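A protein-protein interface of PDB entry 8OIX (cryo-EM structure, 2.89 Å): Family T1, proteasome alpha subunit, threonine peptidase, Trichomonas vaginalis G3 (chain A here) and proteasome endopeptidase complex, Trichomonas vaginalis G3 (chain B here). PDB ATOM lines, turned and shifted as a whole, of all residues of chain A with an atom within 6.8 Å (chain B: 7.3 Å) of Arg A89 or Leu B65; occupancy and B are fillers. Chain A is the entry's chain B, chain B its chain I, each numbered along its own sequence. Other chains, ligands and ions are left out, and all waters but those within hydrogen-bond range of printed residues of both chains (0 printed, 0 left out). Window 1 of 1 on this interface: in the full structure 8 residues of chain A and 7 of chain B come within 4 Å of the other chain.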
ATOM      1  N   VAL A  63     -19.862 -22.866 -23.249  1.00  0.00           N
ATOM      2  CA  VAL A  63     -19.292 -21.648 -22.686  1.00  0.00           C
ATOM      3  C   VAL A  63     -20.003 -21.368 -21.370  1.00  0.00           C
ATOM      4  O   VAL A  63     -21.231 -21.238 -21.334  1.00  0.00           O
ATOM      5  CB  VAL A  63     -19.436 -20.464 -23.652  1.00  0.00           C
ATOM      6  CG1 VAL A  63     -18.940 -19.193 -22.999  1.00  0.00           C
ATOM      7  CG2 VAL A  63     -18.679 -20.729 -24.935  1.00  0.00           C
ATOM      8  N   GLN A  64     -19.237 -21.276 -20.287  1.00  0.00           N
ATOM      9  CA  GLN A  64     -19.813 -21.235 -18.953  1.00  0.00           C
ATOM     10  C   GLN A  64     -19.109 -20.183 -18.111  1.00  0.00           C
ATOM     11  O   GLN A  64     -17.999 -19.744 -18.422  1.00  0.00           O
ATOM     12  CB  GLN A  64     -19.727 -22.603 -18.268  1.00  0.00           C
ATOM     13  CG  GLN A  64     -20.467 -23.715 -18.993  1.00  0.00           C
ATOM     14  CD  GLN A  64     -21.945 -23.741 -18.666  1.00  0.00           C
ATOM     15  OE1 GLN A  64     -22.411 -24.598 -17.916  1.00  0.00           O
ATOM     16  NE2 GLN A  64     -22.694 -22.802 -19.229  1.00  0.00           N
ATOM     17  N   LYS A  65     -19.779 -19.783 -17.034  1.00  0.00           N
ATOM     18  CA  LYS A  65     -19.220 -18.849 -16.068  1.00  0.00           C
ATOM     19  C   LYS A  65     -18.494 -19.615 -14.973  1.00  0.00           C
ATOM     20  O   LYS A  65     -19.028 -20.584 -14.425  1.00  0.00           O
ATOM     21  CB  LYS A  65     -20.319 -17.985 -15.445  1.00  0.00           C
ATOM     22  CG  LYS A  65     -20.492 -16.624 -16.080  1.00  0.00           C
ATOM     23  CD  LYS A  65     -21.575 -15.822 -15.383  1.00  0.00           C
ATOM     24  CE  LYS A  65     -21.166 -15.466 -13.965  1.00  0.00           C
ATOM     25  NZ  LYS A  65     -22.120 -14.512 -13.337  1.00  0.00           N
ATOM     26  N   ILE A  66     -17.278 -19.182 -14.660  1.00  0.00           N
ATOM     27  CA  ILE A  66     -16.609 -19.638 -13.449  1.00  0.00           C
ATOM     28  C   ILE A  66     -16.903 -18.706 -12.284  1.00  0.00           C
ATOM     29  O   ILE A  66     -17.152 -19.157 -11.163  1.00  0.00           O
ATOM     30  CB  ILE A  66     -15.099 -19.768 -13.712  1.00  0.00           C
ATOM     31  CG1 ILE A  66     -14.861 -20.817 -14.795  1.00  0.00           C
ATOM     32  CG2 ILE A  66     -14.365 -20.145 -12.442  1.00  0.00           C
ATOM     33  CD1 ILE A  66     -13.430 -20.966 -15.188  1.00  0.00           C
ATOM     34  N   ASN A  67     -16.891 -17.406 -12.544  1.00  0.00           N
ATOM     35  CA  ASN A  67     -17.316 -16.393 -11.590  1.00  0.00           C
ATOM     36  C   ASN A  67     -17.748 -15.172 -12.394  1.00  0.00           C
ATOM     37  O   ASN A  67     -17.850 -15.228 -13.623  1.00  0.00           O
ATOM     38  CB  ASN A  67     -16.208 -16.085 -10.576  1.00  0.00           C
ATOM     39  CG  ASN A  67     -14.898 -15.701 -11.231  1.00  0.00           C
ATOM     40  OD1 ASN A  67     -14.867 -14.909 -12.169  1.00  0.00           O
ATOM     41  ND2 ASN A  67     -13.804 -16.261 -10.733  1.00  0.00           N
ATOM     42  N   ILE A  72     -15.162 -19.711 -19.124  1.00  0.00           N
ATOM     43  CA  ILE A  72     -14.435 -20.875 -19.619  1.00  0.00           C
ATOM     44  C   ILE A  72     -15.198 -21.509 -20.773  1.00  0.00           C
ATOM     45  O   ILE A  72     -16.429 -21.615 -20.742  1.00  0.00           O
ATOM     46  CB  ILE A  72     -14.186 -21.906 -18.499  1.00  0.00           C
ATOM     47  CG1 ILE A  72     -13.344 -23.073 -19.010  1.00  0.00           C
ATOM     48  CG2 ILE A  72     -15.496 -22.418 -17.938  1.00  0.00           C
ATOM     49  CD1 ILE A  72     -12.869 -23.991 -17.913  1.00  0.00           C
ATOM     50  N   PHE A  81     -15.168 -31.629 -18.750  1.00  0.00           N
ATOM     51  CA  PHE A  81     -15.300 -30.183 -18.643  1.00  0.00           C
ATOM     52  C   PHE A  81     -16.297 -29.800 -17.566  1.00  0.00           C
ATOM     53  O   PHE A  81     -16.084 -28.827 -16.845  1.00  0.00           O
ATOM     54  CB  PHE A  81     -15.731 -29.564 -19.965  1.00  0.00           C
ATOM     55  CG  PHE A  81     -16.304 -28.182 -19.812  1.00  0.00           C
ATOM     56  CD1 PHE A  81     -15.491 -27.117 -19.459  1.00  0.00           C
ATOM     57  CD2 PHE A  81     -17.655 -27.950 -19.995  1.00  0.00           C
ATOM     58  CE1 PHE A  81     -16.010 -25.848 -19.312  1.00  0.00           C
ATOM     59  CE2 PHE A  81     -18.178 -26.681 -19.851  1.00  0.00           C
ATOM     60  CZ  PHE A  81     -17.355 -25.630 -19.507  1.00  0.00           C
ATOM     61  N   HIS A  82     -17.412 -30.523 -17.468  1.00  0.00           N
ATOM     62  CA  HIS A  82     -18.396 -30.186 -16.445  1.00  0.00           C
ATOM     63  C   HIS A  82     -17.831 -30.395 -15.048  1.00  0.00           C
ATOM     64  O   HIS A  82     -18.078 -29.589 -14.144  1.00  0.00           O
ATOM     65  CB  HIS A  82     -19.670 -31.003 -16.642  1.00  0.00           C
ATOM     66  CG  HIS A  82     -20.478 -30.575 -17.824  1.00  0.00           C
ATOM     67  ND1 HIS A  82     -20.862 -29.267 -18.028  1.00  0.00           N
ATOM     68  CD2 HIS A  82     -20.982 -31.281 -18.863  1.00  0.00           C
ATOM     69  CE1 HIS A  82     -21.564 -29.185 -19.144  1.00  0.00           C
ATOM     70  NE2 HIS A  82     -21.652 -30.393 -19.670  1.00  0.00           N
ATOM     71  N   ILE A  84     -14.596 -30.258 -14.194  1.00  0.00           N
ATOM     72  CA  ILE A  84     -13.615 -29.198 -13.969  1.00  0.00           C
ATOM     73  C   ILE A  84     -14.313 -27.866 -13.738  1.00  0.00           C
ATOM     74  O   ILE A  84     -13.853 -27.039 -12.950  1.00  0.00           O
ATOM     75  CB  ILE A  84     -12.619 -29.121 -15.139  1.00  0.00           C
ATOM     76  CG1 ILE A  84     -11.705 -30.339 -15.135  1.00  0.00           C
ATOM     77  CG2 ILE A  84     -11.789 -27.854 -15.062  1.00  0.00           C
ATOM     78  CD1 ILE A  84     -10.980 -30.523 -16.421  1.00  0.00           C
ATOM     79  N   LEU A  85     -15.432 -27.639 -14.423  1.00  0.00           N
ATOM     80  CA  LEU A  85     -16.176 -26.398 -14.269  1.00  0.00           C
ATOM     81  C   LEU A  85     -16.800 -26.295 -12.887  1.00  0.00           C
ATOM     82  O   LEU A  85     -16.760 -25.230 -12.263  1.00  0.00           O
ATOM     83  CB  LEU A  85     -17.251 -26.317 -15.349  1.00  0.00           C
ATOM     84  CG  LEU A  85     -18.283 -25.204 -15.224  1.00  0.00           C
ATOM     85  CD1 LEU A  85     -17.679 -23.860 -15.558  1.00  0.00           C
ATOM     86  CD2 LEU A  85     -19.455 -25.520 -16.126  1.00  0.00           C
ATOM     87  N   LYS A  86     -17.382 -27.389 -12.394  1.00  0.00           N
ATOM     88  CA  LYS A  86     -17.897 -27.386 -11.031  1.00  0.00           C
ATOM     89  C   LYS A  86     -16.775 -27.150 -10.033  1.00  0.00           C
ATOM     90  O   LYS A  86     -16.936 -26.383  -9.077  1.00  0.00           O
ATOM     91  CB  LYS A  86     -18.615 -28.699 -10.727  1.00  0.00           C
ATOM     92  CG  LYS A  86     -19.835 -28.967 -11.586  1.00  0.00           C
ATOM     93  CD  LYS A  86     -21.095 -28.970 -10.746  1.00  0.00           C
ATOM     94  CE  LYS A  86     -21.091 -30.108  -9.743  1.00  0.00           C
ATOM     95  NZ  LYS A  86     -22.340 -30.134  -8.934  1.00  0.00           N
ATOM     96  N   SER A  87     -15.620 -27.786 -10.250  1.00  0.00           N
ATOM     97  CA  SER A  87     -14.491 -27.593  -9.346  1.00  0.00           C
ATOM     98  C   SER A  87     -13.981 -26.157  -9.385  1.00  0.00           C
ATOM     99  O   SER A  87     -13.640 -25.588  -8.346  1.00  0.00           O
ATOM    100  CB  SER A  87     -13.368 -28.563  -9.699  1.00  0.00           C
ATOM    101  OG  SER A  87     -12.559 -28.034 -10.734  1.00  0.00           O
ATOM    102  N   LEU A  88     -13.916 -25.558 -10.574  1.00  0.00           N
ATOM    103  CA  LEU A  88     -13.445 -24.183 -10.700  1.00  0.00           C
ATOM    104  C   LEU A  88     -14.420 -23.198 -10.078  1.00  0.00           C
ATOM    105  O   LEU A  88     -14.004 -22.236  -9.428  1.00  0.00           O
ATOM    106  CB  LEU A  88     -13.207 -23.838 -12.168  1.00  0.00           C
ATOM    107  CG  LEU A  88     -11.936 -24.422 -12.777  1.00  0.00           C
ATOM    108  CD1 LEU A  88     -11.888 -24.164 -14.270  1.00  0.00           C
ATOM    109  CD2 LEU A  88     -10.731 -23.829 -12.083  1.00  0.00           C
ATOM    110  N   ARG A  89     -15.720 -23.409 -10.277  1.00  0.00           N
ATOM    111  CA  ARG A  89     -16.707 -22.549  -9.637  1.00  0.00           C
ATOM    112  C   ARG A  89     -16.655 -22.694  -8.122  1.00  0.00           C
ATOM    113  O   ARG A  89     -16.790 -21.705  -7.391  1.00  0.00           O
ATOM    114  CB  ARG A  89     -18.099 -22.869 -10.175  1.00  0.00           C
ATOM    115  CG  ARG A  89     -18.307 -22.492 -11.624  1.00  0.00           C
ATOM    116  CD  ARG A  89     -19.615 -23.054 -12.135  1.00  0.00           C
ATOM    117  NE  ARG A  89     -20.033 -22.439 -13.387  1.00  0.00           N
ATOM    118  CZ  ARG A  89     -20.935 -22.959 -14.207  1.00  0.00           C
ATOM    119  NH1 ARG A  89     -21.514 -24.118 -13.949  1.00  0.00           N
ATOM    120  NH2 ARG A  89     -21.255 -22.302 -15.318  1.00  0.00           N
ATOM    121  N   LYS A  90     -16.467 -23.922  -7.629  1.00  0.00           N
ATOM    122  CA  LYS A  90     -16.332 -24.130  -6.192  1.00  0.00           C
ATOM    123  C   LYS A  90     -15.069 -23.466  -5.658  1.00  0.00           C
ATOM    124  O   LYS A  90     -15.078 -22.886  -4.569  1.00  0.00           O
ATOM    125  CB  LYS A  90     -16.328 -25.625  -5.880  1.00  0.00           C
ATOM    126  CG  LYS A  90     -16.386 -25.946  -4.398  1.00  0.00           C
ATOM    127  CD  LYS A  90     -16.449 -27.443  -4.162  1.00  0.00           C
ATOM    128  CE  LYS A  90     -15.126 -28.108  -4.495  1.00  0.00           C
ATOM    129  NZ  LYS A  90     -15.103 -29.537  -4.083  1.00  0.00           N
ATOM    130  N   ALA A  91     -13.975 -23.533  -6.416  1.00  0.00           N
ATOM    131  CA  ALA A  91     -12.750 -22.854  -6.015  1.00  0.00           C
ATOM    132  C   ALA A  91     -12.940 -21.345  -6.003  1.00  0.00           C
ATOM    133  O   ALA A  91     -12.414 -20.657  -5.125  1.00  0.00           O
ATOM    134  CB  ALA A  91     -11.604 -23.242  -6.949  1.00  0.00           C
ATOM    135  N   SER A  92     -13.690 -20.815  -6.968  1.00  0.00           N
ATOM    136  CA  SER A  92     -13.946 -19.380  -7.007  1.00  0.00           C
ATOM    137  C   SER A  92     -14.808 -18.937  -5.833  1.00  0.00           C
ATOM    138  O   SER A  92     -14.548 -17.891  -5.229  1.00  0.00           O
ATOM    139  CB  SER A  92     -14.606 -18.998  -8.331  1.00  0.00           C
ATOM    140  OG  SER A  92     -13.725 -19.221  -9.415  1.00  0.00           O
ATOM    141  N   ILE A  93     -15.847 -19.705  -5.498  1.00  0.00           N
ATOM    142  CA  ILE A  93     -16.671 -19.320  -4.357  1.00  0.00           C
ATOM    143  C   ILE A  93     -15.893 -19.482  -3.056  1.00  0.00           C
ATOM    144  O   ILE A  93     -16.075 -18.697  -2.121  1.00  0.00           O
ATOM    145  CB  ILE A  93     -18.013 -20.084  -4.341  1.00  0.00           C
ATOM    146  CG1 ILE A  93     -17.820 -21.594  -4.201  1.00  0.00           C
ATOM    147  CG2 ILE A  93     -18.821 -19.764  -5.591  1.00  0.00           C
ATOM    148  CD1 ILE A  93     -17.885 -22.114  -2.775  1.00  0.00           C
ATOM    149  N   LYS A  94     -15.016 -20.487  -2.964  1.00  0.00           N
ATOM    150  CA  LYS A  94     -14.140 -20.600  -1.801  1.00  0.00           C
ATOM    151  C   LYS A  94     -13.194 -19.409  -1.709  1.00  0.00           C
ATOM    152  O   LYS A  94     -12.932 -18.894  -0.616  1.00  0.00           O
ATOM    153  CB  LYS A  94     -13.348 -21.905  -1.863  1.00  0.00           C
ATOM    154  CG  LYS A  94     -14.108 -23.123  -1.376  1.00  0.00           C
ATOM    155  CD  LYS A  94     -13.235 -24.364  -1.436  1.00  0.00           C
ATOM    156  CE  LYS A  94     -11.998 -24.205  -0.567  1.00  0.00           C
ATOM    157  NZ  LYS A  94     -11.204 -25.461  -0.482  1.00  0.00           N
ATOM    158  N   TYR A  95     -12.656 -18.976  -2.850  1.00  0.00           N
ATOM    159  CA  TYR A  95     -11.791 -17.805  -2.881  1.00  0.00           C
ATOM    160  C   TYR A  95     -12.552 -16.562  -2.448  1.00  0.00           C
ATOM    161  O   TYR A  95     -12.001 -15.693  -1.769  1.00  0.00           O
ATOM    162  CB  TYR A  95     -11.214 -17.631  -4.287  1.00  0.00           C
ATOM    163  CG  TYR A  95     -10.084 -16.633  -4.397  1.00  0.00           C
ATOM    164  CD1 TYR A  95     -10.333 -15.268  -4.414  1.00  0.00           C
ATOM    165  CD2 TYR A  95      -8.768 -17.059  -4.502  1.00  0.00           C
ATOM    166  CE1 TYR A  95      -9.304 -14.359  -4.519  1.00  0.00           C
ATOM    167  CE2 TYR A  95      -7.734 -16.157  -4.613  1.00  0.00           C
ATOM    168  CZ  TYR A  95      -8.008 -14.808  -4.620  1.00  0.00           C
ATOM    169  OH  TYR A  95      -6.980 -13.902  -4.725  1.00  0.00           O
ATOM    170  N   VAL A 108      -7.802 -18.843 -11.253  1.00  0.00           N
ATOM    171  CA  VAL A 108      -8.706 -19.866 -11.773  1.00  0.00           C
ATOM    172  C   VAL A 108      -7.959 -20.804 -12.711  1.00  0.00           C
ATOM    173  O   VAL A 108      -8.119 -22.031 -12.654  1.00  0.00           O
ATOM    174  CB  VAL A 108      -9.907 -19.209 -12.476  1.00  0.00           C
ATOM    175  CG1 VAL A 108     -10.698 -20.251 -13.218  1.00  0.00           C
ATOM    176  CG2 VAL A 108     -10.787 -18.490 -11.475  1.00  0.00           C
ATOM    177  N   HIS A 111      -5.715 -23.065 -10.737  1.00  0.00           N
ATOM    178  CA  HIS A 111      -6.460 -24.102 -10.031  1.00  0.00           C
ATOM    179  C   HIS A 111      -6.905 -25.205 -10.982  1.00  0.00           C
ATOM    180  O   HIS A 111      -6.813 -26.394 -10.651  1.00  0.00           O
ATOM    181  CB  HIS A 111      -7.663 -23.498  -9.310  1.00  0.00           C
ATOM    182  CG  HIS A 111      -8.511 -24.511  -8.605  1.00  0.00           C
ATOM    183  ND1 HIS A 111      -9.418 -25.310  -9.265  1.00  0.00           N
ATOM    184  CD2 HIS A 111      -8.576 -24.865  -7.301  1.00  0.00           C
ATOM    185  CE1 HIS A 111     -10.013 -26.106  -8.396  1.00  0.00           C
ATOM    186  NE2 HIS A 111      -9.520 -25.857  -7.197  1.00  0.00           N
ATOM    187  N   ILE B  59     -23.668 -19.533   2.770  1.00  0.00           N
ATOM    188  CA  ILE B  59     -24.887 -19.942   2.081  1.00  0.00           C
ATOM    189  C   ILE B  59     -25.071 -19.156   0.789  1.00  0.00           C
ATOM    190  O   ILE B  59     -25.598 -19.687  -0.195  1.00  0.00           O
ATOM    191  CB  ILE B  59     -26.097 -19.812   3.021  1.00  0.00           C
ATOM    192  CG1 ILE B  59     -25.898 -20.698   4.256  1.00  0.00           C
ATOM    193  CG2 ILE B  59     -27.382 -20.196   2.309  1.00  0.00           C
ATOM    194  CD1 ILE B  59     -25.184 -22.011   4.002  1.00  0.00           C
ATOM    195  N   SER B  60     -24.637 -17.894   0.753  1.00  0.00           N
ATOM    196  CA  SER B  60     -24.643 -17.153  -0.500  1.00  0.00           C
ATOM    197  C   SER B  60     -23.723 -17.806  -1.518  1.00  0.00           C
ATOM    198  O   SER B  60     -24.061 -17.893  -2.701  1.00  0.00           O
ATOM    199  CB  SER B  60     -24.228 -15.704  -0.252  1.00  0.00           C
ATOM    200  OG  SER B  60     -24.306 -14.943  -1.445  1.00  0.00           O
ATOM    201  N   ALA B  61     -22.555 -18.276  -1.075  1.00  0.00           N
ATOM    202  CA  ALA B  61     -21.657 -18.999  -1.968  1.00  0.00           C
ATOM    203  C   ALA B  61     -22.283 -20.307  -2.433  1.00  0.00           C
ATOM    204  O   ALA B  61     -22.177 -20.665  -3.610  1.00  0.00           O
ATOM    205  CB  ALA B  61     -20.321 -19.259  -1.275  1.00  0.00           C
ATOM    206  N   LYS B  62     -22.932 -21.032  -1.520  1.00  0.00           N
ATOM    207  CA  LYS B  62     -23.581 -22.286  -1.888  1.00  0.00           C
ATOM    208  C   LYS B  62     -24.662 -22.056  -2.932  1.00  0.00           C
ATOM    209  O   LYS B  62     -24.753 -22.796  -3.915  1.00  0.00           O
ATOM    210  CB  LYS B  62     -24.175 -22.963  -0.653  1.00  0.00           C
ATOM    211  CG  LYS B  62     -23.148 -23.511   0.316  1.00  0.00           C
ATOM    212  CD  LYS B  62     -23.813 -24.307   1.423  1.00  0.00           C
ATOM    213  CE  LYS B  62     -22.782 -24.977   2.314  1.00  0.00           C
ATOM    214  NZ  LYS B  62     -21.841 -25.827   1.533  1.00  0.00           N
ATOM    215  N   LEU B  63     -25.480 -21.020  -2.751  1.00  0.00           N
ATOM    216  CA  LEU B  63     -26.556 -20.763  -3.696  1.00  0.00           C
ATOM    217  C   LEU B  63     -26.065 -20.106  -4.977  1.00  0.00           C
ATOM    218  O   LEU B  63     -26.697 -20.279  -6.019  1.00  0.00           O
ATOM    219  CB  LEU B  63     -27.647 -19.917  -3.042  1.00  0.00           C
ATOM    220  CG  LEU B  63     -28.369 -20.671  -1.927  1.00  0.00           C
ATOM    221  CD1 LEU B  63     -29.315 -19.762  -1.192  1.00  0.00           C
ATOM    222  CD2 LEU B  63     -29.112 -21.866  -2.492  1.00  0.00           C
ATOM    223  N   ARG B  64     -24.931 -19.406  -4.941  1.00  0.00           N
ATOM    224  CA  ARG B  64     -24.348 -18.901  -6.178  1.00  0.00           C
ATOM    225  C   ARG B  64     -23.765 -20.050  -6.985  1.00  0.00           C
ATOM    226  O   ARG B  64     -23.918 -20.101  -8.210  1.00  0.00           O
ATOM    227  CB  ARG B  64     -23.282 -17.850  -5.868  1.00  0.00           C
ATOM    228  CG  ARG B  64     -22.214 -17.699  -6.938  1.00  0.00           C
ATOM    229  CD  ARG B  64     -21.310 -16.511  -6.651  1.00  0.00           C
ATOM    230  NE  ARG B  64     -21.733 -15.308  -7.357  1.00  0.00           N
ATOM    231  CZ  ARG B  64     -21.733 -15.161  -8.675  1.00  0.00           C
ATOM    232  NH1 ARG B  64     -21.064 -15.986  -9.464  1.00  0.00           N
ATOM    233  NH2 ARG B  64     -22.344 -14.107  -9.209  1.00  0.00           N
ATOM    234  N   LEU B  65     -23.143 -21.010  -6.301  1.00  0.00           N
ATOM    235  CA  LEU B  65     -22.645 -22.205  -6.969  1.00  0.00           C
ATOM    236  C   LEU B  65     -23.802 -23.034  -7.503  1.00  0.00           C
ATOM    237  O   LEU B  65     -23.714 -23.614  -8.590  1.00  0.00           O
ATOM    238  CB  LEU B  65     -21.801 -23.013  -5.984  1.00  0.00           C
ATOM    239  CG  LEU B  65     -21.031 -24.242  -6.452  1.00  0.00           C
ATOM    240  CD1 LEU B  65     -20.155 -23.886  -7.618  1.00  0.00           C
ATOM    241  CD2 LEU B  65     -20.200 -24.798  -5.309  1.00  0.00           C
ATOM    242  N   PHE B  66     -24.909 -23.066  -6.761  1.00  0.00           N
ATOM    243  CA  PHE B  66     -26.112 -23.756  -7.206  1.00  0.00           C
ATOM    244  C   PHE B  66     -26.658 -23.109  -8.473  1.00  0.00           C
ATOM    245  O   PHE B  66     -26.920 -23.786  -9.471  1.00  0.00           O
ATOM    246  CB  PHE B  66     -27.142 -23.740  -6.075  1.00  0.00           C
ATOM    247  CG  PHE B  66     -28.465 -24.347  -6.435  1.00  0.00           C
ATOM    248  CD1 PHE B  66     -28.688 -25.698  -6.242  1.00  0.00           C
ATOM    249  CD2 PHE B  66     -29.493 -23.566  -6.932  1.00  0.00           C
ATOM    250  CE1 PHE B  66     -29.902 -26.261  -6.556  1.00  0.00           C
ATOM    251  CE2 PHE B  66     -30.710 -24.126  -7.252  1.00  0.00           C
ATOM    252  CZ  PHE B  66     -30.915 -25.475  -7.064  1.00  0.00           C
ATOM    253  N   GLN B  67     -26.865 -21.790  -8.437  1.00  0.00           N
ATOM    254  CA  GLN B  67     -27.399 -21.080  -9.591  1.00  0.00           C
ATOM    255  C   GLN B  67     -26.462 -21.162 -10.789  1.00  0.00           C
ATOM    256  O   GLN B  67     -26.917 -21.123 -11.936  1.00  0.00           O
ATOM    257  CB  GLN B  67     -27.665 -19.619  -9.222  1.00  0.00           C
ATOM    258  CG  GLN B  67     -28.214 -18.774 -10.358  1.00  0.00           C
ATOM    259  CD  GLN B  67     -29.142 -17.682  -9.871  1.00  0.00           C
ATOM    260  OE1 GLN B  67     -28.969 -17.149  -8.776  1.00  0.00           O
ATOM    261  NE2 GLN B  67     -30.138 -17.346 -10.681  1.00  0.00           N
ATOM    262  N   MET B  68     -25.154 -21.276 -10.553  1.00  0.00           N
ATOM    263  CA  MET B  68     -24.218 -21.419 -11.662  1.00  0.00           C
ATOM    264  C   MET B  68     -24.295 -22.814 -12.276  1.00  0.00           C
ATOM    265  O   MET B  68     -24.525 -22.961 -13.481  1.00  0.00           O
ATOM    266  CB  MET B  68     -22.796 -21.107 -11.195  1.00  0.00           C
ATOM    267  CG  MET B  68     -22.505 -19.622 -11.069  1.00  0.00           C
ATOM    268  SD  MET B  68     -20.759 -19.258 -10.823  1.00  0.00           S
ATOM    269  CE  MET B  68     -20.469 -20.046  -9.242  1.00  0.00           C
ATOM    270  N   ASN B  69     -24.096 -23.852 -11.460  1.00  0.00           N
ATOM    271  CA  ASN B  69     -24.094 -25.216 -11.981  1.00  0.00           C
ATOM    272  C   ASN B  69     -25.441 -25.581 -12.592  1.00  0.00           C
ATOM    273  O   ASN B  69     -25.507 -26.131 -13.697  1.00  0.00           O
ATOM    274  CB  ASN B  69     -23.730 -26.205 -10.874  1.00  0.00           C
ATOM    275  CG  ASN B  69     -22.415 -25.874 -10.206  1.00  0.00           C
ATOM    276  OD1 ASN B  69     -22.288 -25.953  -8.986  1.00  0.00           O
ATOM    277  ND2 ASN B  69     -21.425 -25.504 -11.005  1.00  0.00           N
ATOM    278  N   THR B  70     -26.527 -25.279 -11.887  1.00  0.00           N
ATOM    279  CA  THR B  70     -27.857 -25.732 -12.259  1.00  0.00           C
ATOM    280  C   THR B  70     -28.653 -24.705 -13.052  1.00  0.00           C
ATOM    281  O   THR B  70     -29.696 -25.058 -13.613  1.00  0.00           O
ATOM    282  CB  THR B  70     -28.638 -26.113 -11.000  1.00  0.00           C
ATOM    283  OG1 THR B  70     -29.006 -24.924 -10.292  1.00  0.00           O
ATOM    284  CG2 THR B  70     -27.770 -26.966 -10.093  1.00  0.00           C
ATOM    285  N   GLY B  71     -28.197 -23.456 -13.116  1.00  0.00           N
ATOM    286  CA  GLY B  71     -28.958 -22.425 -13.794  1.00  0.00           C
ATOM    287  C   GLY B  71     -30.288 -22.102 -13.156  1.00  0.00           C
ATOM    288  O   GLY B  71     -31.143 -21.492 -13.801  1.00  0.00           O
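The backbone carbonyl oxygen (O) of Lys A65 is in hydrogen-bond range of the guanidinium group (NH2) of Arg A89, 3.0 Å away. The guanidinium group of Arg B64 sits at hydrogen-bond distance from the side-chain sulfur of Met B68, at 3.6 Å. The side-chain amide oxygen of Asn B69 lies close to the backbone carbonyl oxygen of Leu B65 (2.8 Å).
Among the printed residues, merely in contact across the chains: Lys A86 with Asn B69 (3.4 Å), Arg A89 with Leu B65 (3.4 Å), Lys A90 with Leu B65 (3.7 Å) and Ile A93 with Ala B61 (3.9 Å).
NH1 of Arg A89 is in hydrogen-bond range of O of Met B68 (3.3 Å). ND2 of Asn B69 lies close to NH1 of Arg A89, 3.3 Å away. The side-chain sulfur (SD) of Met B68 sits close to the backbone carbonyl oxygen (O) of Ile A66 (3.6 Å).
Printed residues of chain B that touch a printed residue of chain A: Ala B61, Leu B65, Met B68 and Asn B69. Hydrophobic or aromatic side chains of chain B within 4 Å of the printed part of chain A: Ala B61, Leu B65 and Met B68. Among the printed residues, 7 pairs touch across the chains.
Asn A67 touches none of the printed residues of chain B. Of chain B, only Leu B65 (3.4 Å), Met B68 (3.3 Å) and Asn B69 (3.2 Å) come within 4 Å of Arg A89. Of the printed residues of chain B, Lys A90 touches Leu B65 (3.7 Å). Printed residues of chain B within 4 Å of Ile A93: Ala B61. Printed residues of chain A within 4 Å of Ala B61: Ile A93 (3.9 Å). Leu B65 touches just these residues of chain A: Arg A89 (3.4 Å) and Lys A90 (3.7 Å). The nearest residue of chain B that does not touch Arg A89 is Thr B70 (5.5 Å). The nearest residue of chain A that does not touch Leu B65 is Ile A93 (4.1 Å).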
